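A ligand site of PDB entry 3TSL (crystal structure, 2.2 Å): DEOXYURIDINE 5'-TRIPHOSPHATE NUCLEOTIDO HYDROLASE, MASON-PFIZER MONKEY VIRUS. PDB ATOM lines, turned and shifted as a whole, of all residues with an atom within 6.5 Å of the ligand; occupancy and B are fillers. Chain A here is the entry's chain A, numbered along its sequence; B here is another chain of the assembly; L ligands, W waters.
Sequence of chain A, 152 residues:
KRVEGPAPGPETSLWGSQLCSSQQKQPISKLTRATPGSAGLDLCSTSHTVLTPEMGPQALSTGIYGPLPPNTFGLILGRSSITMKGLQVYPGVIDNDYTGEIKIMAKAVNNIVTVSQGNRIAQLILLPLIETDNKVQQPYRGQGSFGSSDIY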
ATOM      1  N   ILE A  76      -9.791 -16.423  24.937  1.00  0.00           N
ATOM      2  CA  ILE A  76      -9.429 -17.600  24.150  1.00  0.00           C
ATOM      3  C   ILE A  76      -9.180 -18.761  25.093  1.00  0.00           C
ATOM      4  O   ILE A  76      -8.404 -18.648  26.041  1.00  0.00           O
ATOM      5  CB  ILE A  76      -8.176 -17.369  23.231  1.00  0.00           C
ATOM      6  CG1 ILE A  76      -8.439 -16.276  22.229  1.00  0.00           C
ATOM      7  CG2 ILE A  76      -7.805 -18.605  22.468  1.00  0.00           C
ATOM      8  CD1 ILE A  76      -7.173 -15.984  21.463  1.00  0.00           C
ATOM      9  N   TYR A  90      -3.310 -21.951  26.027  1.00  0.00           N
ATOM     10  CA  TYR A  90      -3.221 -21.078  27.203  1.00  0.00           C
ATOM     11  C   TYR A  90      -4.295 -20.014  27.133  1.00  0.00           C
ATOM     12  O   TYR A  90      -4.428 -19.354  26.104  1.00  0.00           O
ATOM     13  CB  TYR A  90      -1.893 -20.387  27.206  1.00  0.00           C
ATOM     14  CG  TYR A  90      -0.739 -21.345  27.374  1.00  0.00           C
ATOM     15  CD1 TYR A  90      -0.550 -22.040  28.576  1.00  0.00           C
ATOM     16  CD2 TYR A  90       0.166 -21.553  26.348  1.00  0.00           C
ATOM     17  CE1 TYR A  90       0.548 -22.920  28.726  1.00  0.00           C
ATOM     18  CE2 TYR A  90       1.272 -22.406  26.510  1.00  0.00           C
ATOM     19  CZ  TYR A  90       1.448 -23.086  27.703  1.00  0.00           C
ATOM     20  OH  TYR A  90       2.531 -23.952  27.845  1.00  0.00           O
ATOM     21  N   PRO A  91      -5.063 -19.825  28.235  1.00  0.00           N
ATOM     22  CA  PRO A  91      -6.119 -18.810  28.237  1.00  0.00           C
ATOM     23  C   PRO A  91      -5.580 -17.439  27.738  1.00  0.00           C
ATOM     24  O   PRO A  91      -4.562 -16.982  28.210  1.00  0.00           O
ATOM     25  CB  PRO A  91      -6.527 -18.724  29.704  1.00  0.00           C
ATOM     26  CG  PRO A  91      -6.150 -20.047  30.304  1.00  0.00           C
ATOM     27  CD  PRO A  91      -5.012 -20.596  29.499  1.00  0.00           C
ATOM     28  N   GLY A  92      -6.273 -16.791  26.814  1.00  0.00           N
ATOM     29  CA  GLY A  92      -5.821 -15.493  26.401  1.00  0.00           C
ATOM     30  C   GLY A  92      -6.931 -14.469  26.438  1.00  0.00           C
ATOM     31  O   GLY A  92      -8.101 -14.774  26.182  1.00  0.00           O
ATOM     32  N   VAL A  93      -6.549 -13.243  26.752  1.00  0.00           N
ATOM     33  CA  VAL A  93      -7.472 -12.136  26.879  1.00  0.00           C
ATOM     34  C   VAL A  93      -7.347 -11.276  25.607  1.00  0.00           C
ATOM     35  O   VAL A  93      -6.220 -10.841  25.240  1.00  0.00           O
ATOM     36  CB  VAL A  93      -7.074 -11.352  28.122  1.00  0.00           C
ATOM     37  CG1 VAL A  93      -7.748 -10.016  28.176  1.00  0.00           C
ATOM     38  CG2 VAL A  93      -7.384 -12.192  29.361  1.00  0.00           C
ATOM     39  N   ILE A  94      -8.477 -11.107  24.888  1.00  0.00           N
ATOM     40  CA  ILE A  94      -8.519 -10.161  23.772  1.00  0.00           C
ATOM     41  C   ILE A  94      -9.192  -8.865  24.223  1.00  0.00           C
ATOM     42  O   ILE A  94     -10.362  -8.850  24.640  1.00  0.00           O
ATOM     43  CB  ILE A  94      -9.292 -10.680  22.532  1.00  0.00           C
ATOM     44  CG1 ILE A  94      -9.013 -12.156  22.271  1.00  0.00           C
ATOM     45  CG2 ILE A  94      -8.932  -9.857  21.330  1.00  0.00           C
ATOM     46  CD1 ILE A  94      -7.544 -12.537  22.350  1.00  0.00           C
ATOM     47  N   ASP A  95      -8.473  -7.762  24.122  1.00  0.00           N
ATOM     48  CA  ASP A  95      -9.089  -6.505  24.539  1.00  0.00           C
ATOM     49  C   ASP A  95     -10.037  -5.945  23.498  1.00  0.00           C
ATOM     50  O   ASP A  95      -9.923  -6.229  22.268  1.00  0.00           O
ATOM     51  CB  ASP A  95      -8.043  -5.474  24.925  1.00  0.00           C
ATOM     52  CG  ASP A  95      -7.090  -6.010  25.965  1.00  0.00           C
ATOM     53  OD1 ASP A  95      -7.585  -6.397  27.032  1.00  0.00           O
ATOM     54  OD2 ASP A  95      -5.877  -6.109  25.678  1.00  0.00           O
ATOM     55  N   ASN A  96     -10.971  -5.148  23.990  1.00  0.00           N
ATOM     56  CA  ASN A  96     -12.035  -4.677  23.163  1.00  0.00           C
ATOM     57  C   ASN A  96     -11.526  -3.970  21.919  1.00  0.00           C
ATOM     58  O   ASN A  96     -12.102  -4.070  20.812  1.00  0.00           O
ATOM     59  CB  ASN A  96     -12.945  -3.762  23.971  1.00  0.00           C
ATOM     60  CG  ASN A  96     -14.106  -3.306  23.183  1.00  0.00           C
ATOM     61  OD1 ASN A  96     -14.049  -2.270  22.542  1.00  0.00           O
ATOM     62  ND2 ASN A  96     -15.152  -4.103  23.160  1.00  0.00           N
ATOM     63  N   ASP A  97     -10.428  -3.266  22.104  1.00  0.00           N
ATOM     64  CA  ASP A  97      -9.940  -2.345  21.081  1.00  0.00           C
ATOM     65  C   ASP A  97      -8.727  -2.949  20.381  1.00  0.00           C
ATOM     66  O   ASP A  97      -7.999  -2.245  19.700  1.00  0.00           O
ATOM     67  CB  ASP A  97      -9.537  -0.988  21.715  1.00  0.00           C
ATOM     68  CG  ASP A  97      -8.529  -1.150  22.919  1.00  0.00           C
ATOM     69  OD1 ASP A  97      -8.101  -2.286  23.282  1.00  0.00           O
ATOM     70  OD2 ASP A  97      -8.159  -0.110  23.510  1.00  0.00           O
ATOM     71  N   TYR A  98      -8.472  -4.246  20.576  1.00  0.00           N
ATOM     72  CA  TYR A  98      -7.381  -4.883  19.882  1.00  0.00           C
ATOM     73  C   TYR A  98      -7.736  -4.981  18.391  1.00  0.00           C
ATOM     74  O   TYR A  98      -8.864  -5.409  18.025  1.00  0.00           O
ATOM     75  CB  TYR A  98      -7.181  -6.260  20.448  1.00  0.00           C
ATOM     76  CG  TYR A  98      -6.093  -7.074  19.789  1.00  0.00           C
ATOM     77  CD1 TYR A  98      -4.745  -6.684  19.853  1.00  0.00           C
ATOM     78  CD2 TYR A  98      -6.422  -8.260  19.133  1.00  0.00           C
ATOM     79  CE1 TYR A  98      -3.735  -7.473  19.261  1.00  0.00           C
ATOM     80  CE2 TYR A  98      -5.436  -9.064  18.553  1.00  0.00           C
ATOM     81  CZ  TYR A  98      -4.103  -8.642  18.603  1.00  0.00           C
ATOM     82  OH  TYR A  98      -3.135  -9.422  18.027  1.00  0.00           O
ATOM     83  N   GLY A 100      -5.393  -6.179  16.005  1.00  0.00           N
ATOM     84  CA  GLY A 100      -4.491  -7.096  15.346  1.00  0.00           C
ATOM     85  C   GLY A 100      -5.089  -8.481  15.266  1.00  0.00           C
ATOM     86  O   GLY A 100      -6.281  -8.692  15.524  1.00  0.00           O
ATOM     87  N   GLU A 101      -4.238  -9.434  14.886  1.00  0.00           N
ATOM     88  CA  GLU A 101      -4.668 -10.762  14.580  1.00  0.00           C
ATOM     89  C   GLU A 101      -4.738 -11.529  15.853  1.00  0.00           C
ATOM     90  O   GLU A 101      -3.858 -11.385  16.693  1.00  0.00           O
ATOM     91  CB  GLU A 101      -3.701 -11.470  13.651  1.00  0.00           C
ATOM     92  CG  GLU A 101      -4.258 -12.808  13.154  1.00  0.00           C
ATOM     93  CD  GLU A 101      -3.219 -13.636  12.436  1.00  0.00           C
ATOM     94  OE1 GLU A 101      -2.134 -13.077  12.179  1.00  0.00           O
ATOM     95  OE2 GLU A 101      -3.477 -14.828  12.138  1.00  0.00           O
ATOM     96  N   ILE A 102      -5.791 -12.326  16.001  1.00  0.00           N
ATOM     97  CA  ILE A 102      -6.025 -13.125  17.152  1.00  0.00           C
ATOM     98  C   ILE A 102      -5.209 -14.374  16.931  1.00  0.00           C
ATOM     99  O   ILE A 102      -5.453 -15.152  15.982  1.00  0.00           O
ATOM    100  CB  ILE A 102      -7.530 -13.457  17.313  1.00  0.00           C
ATOM    101  CG1 ILE A 102      -8.216 -12.275  17.980  1.00  0.00           C
ATOM    102  CG2 ILE A 102      -7.735 -14.695  18.199  1.00  0.00           C
ATOM    103  CD1 ILE A 102      -9.625 -12.066  17.594  1.00  0.00           C
ATOM    104  N   LYS A 103      -4.236 -14.548  17.810  1.00  0.00           N
ATOM    105  CA  LYS A 103      -3.446 -15.760  17.792  1.00  0.00           C
ATOM    106  C   LYS A 103      -3.809 -16.655  18.979  1.00  0.00           C
ATOM    107  O   LYS A 103      -4.213 -16.165  20.069  1.00  0.00           O
ATOM    108  CB  LYS A 103      -1.980 -15.353  17.756  1.00  0.00           C
ATOM    109  CG  LYS A 103      -1.622 -14.744  16.371  1.00  0.00           C
ATOM    110  CD  LYS A 103      -0.217 -14.268  16.314  1.00  0.00           C
ATOM    111  CE  LYS A 103       0.272 -14.261  14.887  1.00  0.00           C
ATOM    112  NZ  LYS A 103       1.608 -14.936  14.814  1.00  0.00           N
ATOM    113  N   ILE A 104      -3.687 -17.957  18.767  1.00  0.00           N
ATOM    114  CA  ILE A 104      -3.900 -18.960  19.787  1.00  0.00           C
ATOM    115  C   ILE A 104      -2.551 -19.349  20.378  1.00  0.00           C
ATOM    116  O   ILE A 104      -1.628 -19.770  19.637  1.00  0.00           O
ATOM    117  CB  ILE A 104      -4.532 -20.225  19.201  1.00  0.00           C
ATOM    118  CG1 ILE A 104      -5.829 -19.893  18.461  1.00  0.00           C
ATOM    119  CG2 ILE A 104      -4.786 -21.270  20.284  1.00  0.00           C
ATOM    120  CD1 ILE A 104      -6.219 -20.990  17.478  1.00  0.00           C
ATOM    121  N   MET A 105      -2.416 -19.237  21.687  1.00  0.00           N
ATOM    122  CA  MET A 105      -1.145 -19.616  22.320  1.00  0.00           C
ATOM    123  C   MET A 105      -1.236 -21.066  22.767  1.00  0.00           C
ATOM    124  O   MET A 105      -2.041 -21.408  23.644  1.00  0.00           O
ATOM    125  CB  MET A 105      -0.813 -18.695  23.467  1.00  0.00           C
ATOM    126  CG  MET A 105      -0.743 -17.262  23.085  1.00  0.00           C
ATOM    127  SD  MET A 105      -0.331 -16.317  24.549  1.00  0.00           S
ATOM    128  CE  MET A 105      -1.791 -16.482  25.588  1.00  0.00           C
ATOM    129  N   SER B  38      -8.356  -2.087  27.628  1.00  0.00           N
ATOM    130  CA  SER B  38      -7.821  -3.215  28.352  1.00  0.00           C
ATOM    131  C   SER B  38      -8.883  -3.861  29.198  1.00  0.00           C
ATOM    132  O   SER B  38      -9.492  -3.196  30.004  1.00  0.00           O
ATOM    133  CB  SER B  38      -6.678  -2.780  29.241  1.00  0.00           C
ATOM    134  OG  SER B  38      -5.493  -2.737  28.501  1.00  0.00           O
ATOM    135  N   ASP B  42      -3.460  -4.724  35.580  1.00  0.00           N
ATOM    136  CA  ASP B  42      -2.117  -5.279  35.658  1.00  0.00           C
ATOM    137  C   ASP B  42      -1.647  -5.615  37.066  1.00  0.00           C
ATOM    138  O   ASP B  42      -1.809  -4.818  37.990  1.00  0.00           O
ATOM    139  CB  ASP B  42      -1.115  -4.398  34.914  1.00  0.00           C
ATOM    140  CG  ASP B  42      -1.213  -4.599  33.408  1.00  0.00           C
ATOM    141  OD1 ASP B  42      -1.618  -5.697  32.983  1.00  0.00           O
ATOM    142  OD2 ASP B  42      -0.871  -3.691  32.652  1.00  0.00           O
ATOM    143  N   GLY B  78      -2.784 -14.936  32.667  1.00  0.00           N
ATOM    144  CA  GLY B  78      -1.457 -14.446  32.297  1.00  0.00           C
ATOM    145  C   GLY B  78      -1.565 -13.341  31.256  1.00  0.00           C
ATOM    146  O   GLY B  78      -2.640 -13.055  30.730  1.00  0.00           O
ATOM    147  N   ARG B  79      -0.437 -12.704  30.971  1.00  0.00           N
ATOM    148  CA  ARG B  79      -0.358 -11.765  29.900  1.00  0.00           C
ATOM    149  C   ARG B  79       0.196 -12.553  28.727  1.00  0.00           C
ATOM    150  O   ARG B  79       0.958 -13.493  28.959  1.00  0.00           O
ATOM    151  CB  ARG B  79       0.576 -10.635  30.308  1.00  0.00           C
ATOM    152  CG  ARG B  79      -0.049  -9.732  31.333  1.00  0.00           C
ATOM    153  N   SER B  80      -0.181 -12.235  27.484  1.00  0.00           N
ATOM    154  CA  SER B  80       0.392 -13.016  26.350  1.00  0.00           C
ATOM    155  C   SER B  80       1.900 -12.991  26.234  1.00  0.00           C
ATOM    156  O   SER B  80       2.493 -14.015  25.948  1.00  0.00           O
ATOM    157  CB  SER B  80      -0.217 -12.636  25.004  1.00  0.00           C
ATOM    158  OG  SER B  80      -0.651 -11.295  25.068  1.00  0.00           O
ATOM    159  N   SER B  81       2.543 -11.842  26.446  1.00  0.00           N
ATOM    160  CA  SER B  81       3.991 -11.809  26.244  1.00  0.00           C
ATOM    161  C   SER B  81       4.733 -12.651  27.241  1.00  0.00           C
ATOM    162  O   SER B  81       5.754 -13.268  26.906  1.00  0.00           O
ATOM    163  CB  SER B  81       4.577 -10.381  26.175  1.00  0.00           C
ATOM    164  OG  SER B  81       3.833  -9.526  26.964  1.00  0.00           O
ATOM    165  N   ILE B  82       4.217 -12.682  28.461  1.00  0.00           N
ATOM    166  CA  ILE B  82       4.834 -13.461  29.518  1.00  0.00           C
ATOM    167  C   ILE B  82       4.689 -14.961  29.266  1.00  0.00           C
ATOM    168  O   ILE B  82       5.682 -15.710  29.365  1.00  0.00           O
ATOM    169  CB  ILE B  82       4.273 -13.035  30.887  1.00  0.00           C
ATOM    170  CG1 ILE B  82       4.831 -11.637  31.265  1.00  0.00           C
ATOM    171  CG2 ILE B  82       4.661 -14.027  31.929  1.00  0.00           C
ATOM    172  N   GLN B 123      -2.830 -10.470  34.918  1.00  0.00           N
ATOM    173  CA  GLN B 123      -3.873  -9.466  34.843  1.00  0.00           C
ATOM    174  C   GLN B 123      -5.089  -9.980  35.627  1.00  0.00           C
ATOM    175  O   GLN B 123      -5.338 -11.183  35.738  1.00  0.00           O
ATOM    176  CB  GLN B 123      -4.160  -9.079  33.384  1.00  0.00           C
ATOM    177  CG  GLN B 123      -4.704 -10.159  32.568  1.00  0.00           C
ATOM    178  CD  GLN B 123      -4.705  -9.771  31.138  1.00  0.00           C
ATOM    179  OE1 GLN B 123      -5.330  -8.768  30.740  1.00  0.00           O
ATOM    180  NE2 GLN B 123      -4.001 -10.544  30.325  1.00  0.00           N
HETATM  181  N1  LIG L   1      -3.811 -11.843  22.213  1.00  0.00           N
HETATM  182  C1  LIG L   1      -4.103 -12.862  21.331  1.00  0.00           C
HETATM  183  N2  LIG L   1      -4.211 -14.162  21.773  1.00  0.00           N
HETATM  184  C2  LIG L   1      -4.057 -14.454  23.107  1.00  0.00           C
HETATM  185  C3  LIG L   1      -3.757 -13.441  23.988  1.00  0.00           C
HETATM  186  C4  LIG L   1      -3.640 -12.127  23.532  1.00  0.00           C
HETATM  187  O1  LIG L   1      -4.236 -12.651  20.124  1.00  0.00           O
HETATM  188  O2  LIG L   1      -4.166 -15.616  23.489  1.00  0.00           O
HETATM  189  C5  LIG L   1      -3.687 -10.451  21.752  1.00  0.00           C
HETATM  190  C6  LIG L   1      -5.036  -9.791  22.087  1.00  0.00           C
HETATM  191  C7  LIG L   1      -4.724  -8.898  23.242  1.00  0.00           C
HETATM  192  C8  LIG L   1      -3.269  -8.543  22.949  1.00  0.00           C
HETATM  193  O3  LIG L   1      -5.585  -7.768  23.260  1.00  0.00           O
HETATM  194  O4  LIG L   1      -2.689  -9.727  22.442  1.00  0.00           O
HETATM  195  C9  LIG L   1      -2.470  -8.159  24.180  1.00  0.00           C
HETATM  196  O5  LIG L   1      -2.557  -9.282  25.012  1.00  0.00           O
HETATM  197  P1  LIG L   1      -2.096  -9.231  26.574  1.00  0.00           P
HETATM  198  O6  LIG L   1      -0.584  -9.173  26.600  1.00  0.00           O
HETATM  199  O7  LIG L   1      -2.628  -7.954  27.199  1.00  0.00           O
HETATM  200  O8  LIG L   1      -2.657 -10.388  27.294  1.00  0.00           O
HETATM  201  O   HOH W   1      -4.453 -18.251  23.535  1.00  0.00           O
HETATM  202  O   HOH W   2       0.236  -9.374  20.709  1.00  0.00           O
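An oxygen (O8) of the ligand lies within hydrogen-bond range of the backbone NH of Ser 80 of chain B, at 3.1 Å. The side-chain hydroxyl of Ser 80 of chain B is in hydrogen-bond range of an oxygen (O6) of the ligand (2.6 Å). N of Lys 103 is in hydrogen-bond range of O1 of the ligand (3.0 Å). The backbone carbonyl oxygen of Lys 103 lies within hydrogen-bond range of a nitrogen (N2) of the ligand (2.6 Å). The backbone NH of Asp 95 is in hydrogen-bond range of an oxygen (O3) of the ligand (3.0 Å). O3 of the ligand sits at hydrogen-bond distance from OD2 of Asp 95 (2.9 Å). The side-chain amide nitrogen (NE2) of Gln 123 of chain B lies within hydrogen-bond range of an oxygen (O8) of the ligand (3.3 Å).
N of Tyr 90 lies within hydrogen-bond range of O of Met 105 (2.8 Å). O of Gly 78 of chain B is in hydrogen-bond range of NE2 of Gln 123 of chain B, at 2.9 Å. O of Gly 92 sits at hydrogen-bond distance from N of Ile 76 (2.7 Å). The side-chain hydroxyl (OH) of Tyr 98 is in hydrogen-bond range of the backbone carbonyl oxygen (O) of Glu 101, 2.5 Å away.
Ile 76 touches the ligand. CA of Gly 92 touches O2 of the ligand (3.4 Å). O of Val 93 touches C7 of the ligand (3.2 Å). Ile 94 touches the ligand. CB of Tyr 98 touches O3 of the ligand, at 3.6 Å. O of Glu 101 touches O1 of the ligand (3.7 Å). Ile 102 touches the ligand. Met 105 touches the ligand. Arg 79 of chain B touches the ligand (CA to O8, 3.7 Å). Within 4 Å of the ligand: Ile 76, Gly 92, Val 93, Ile 94, Asp 95, Tyr 98, Glu 101, Ile 102, Lys 103, Met 105, Arg 79 of chain B, Ser 80 of chain B and Gln 123 of chain B.
Water W1 lies within hydrogen-bond range of an oxygen (O2) of the ligand (2.7 Å), the backbone carbonyl oxygen (O) of Tyr 90 (2.8 Å) and the backbone NH (N) of Met 105 (2.9 Å).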
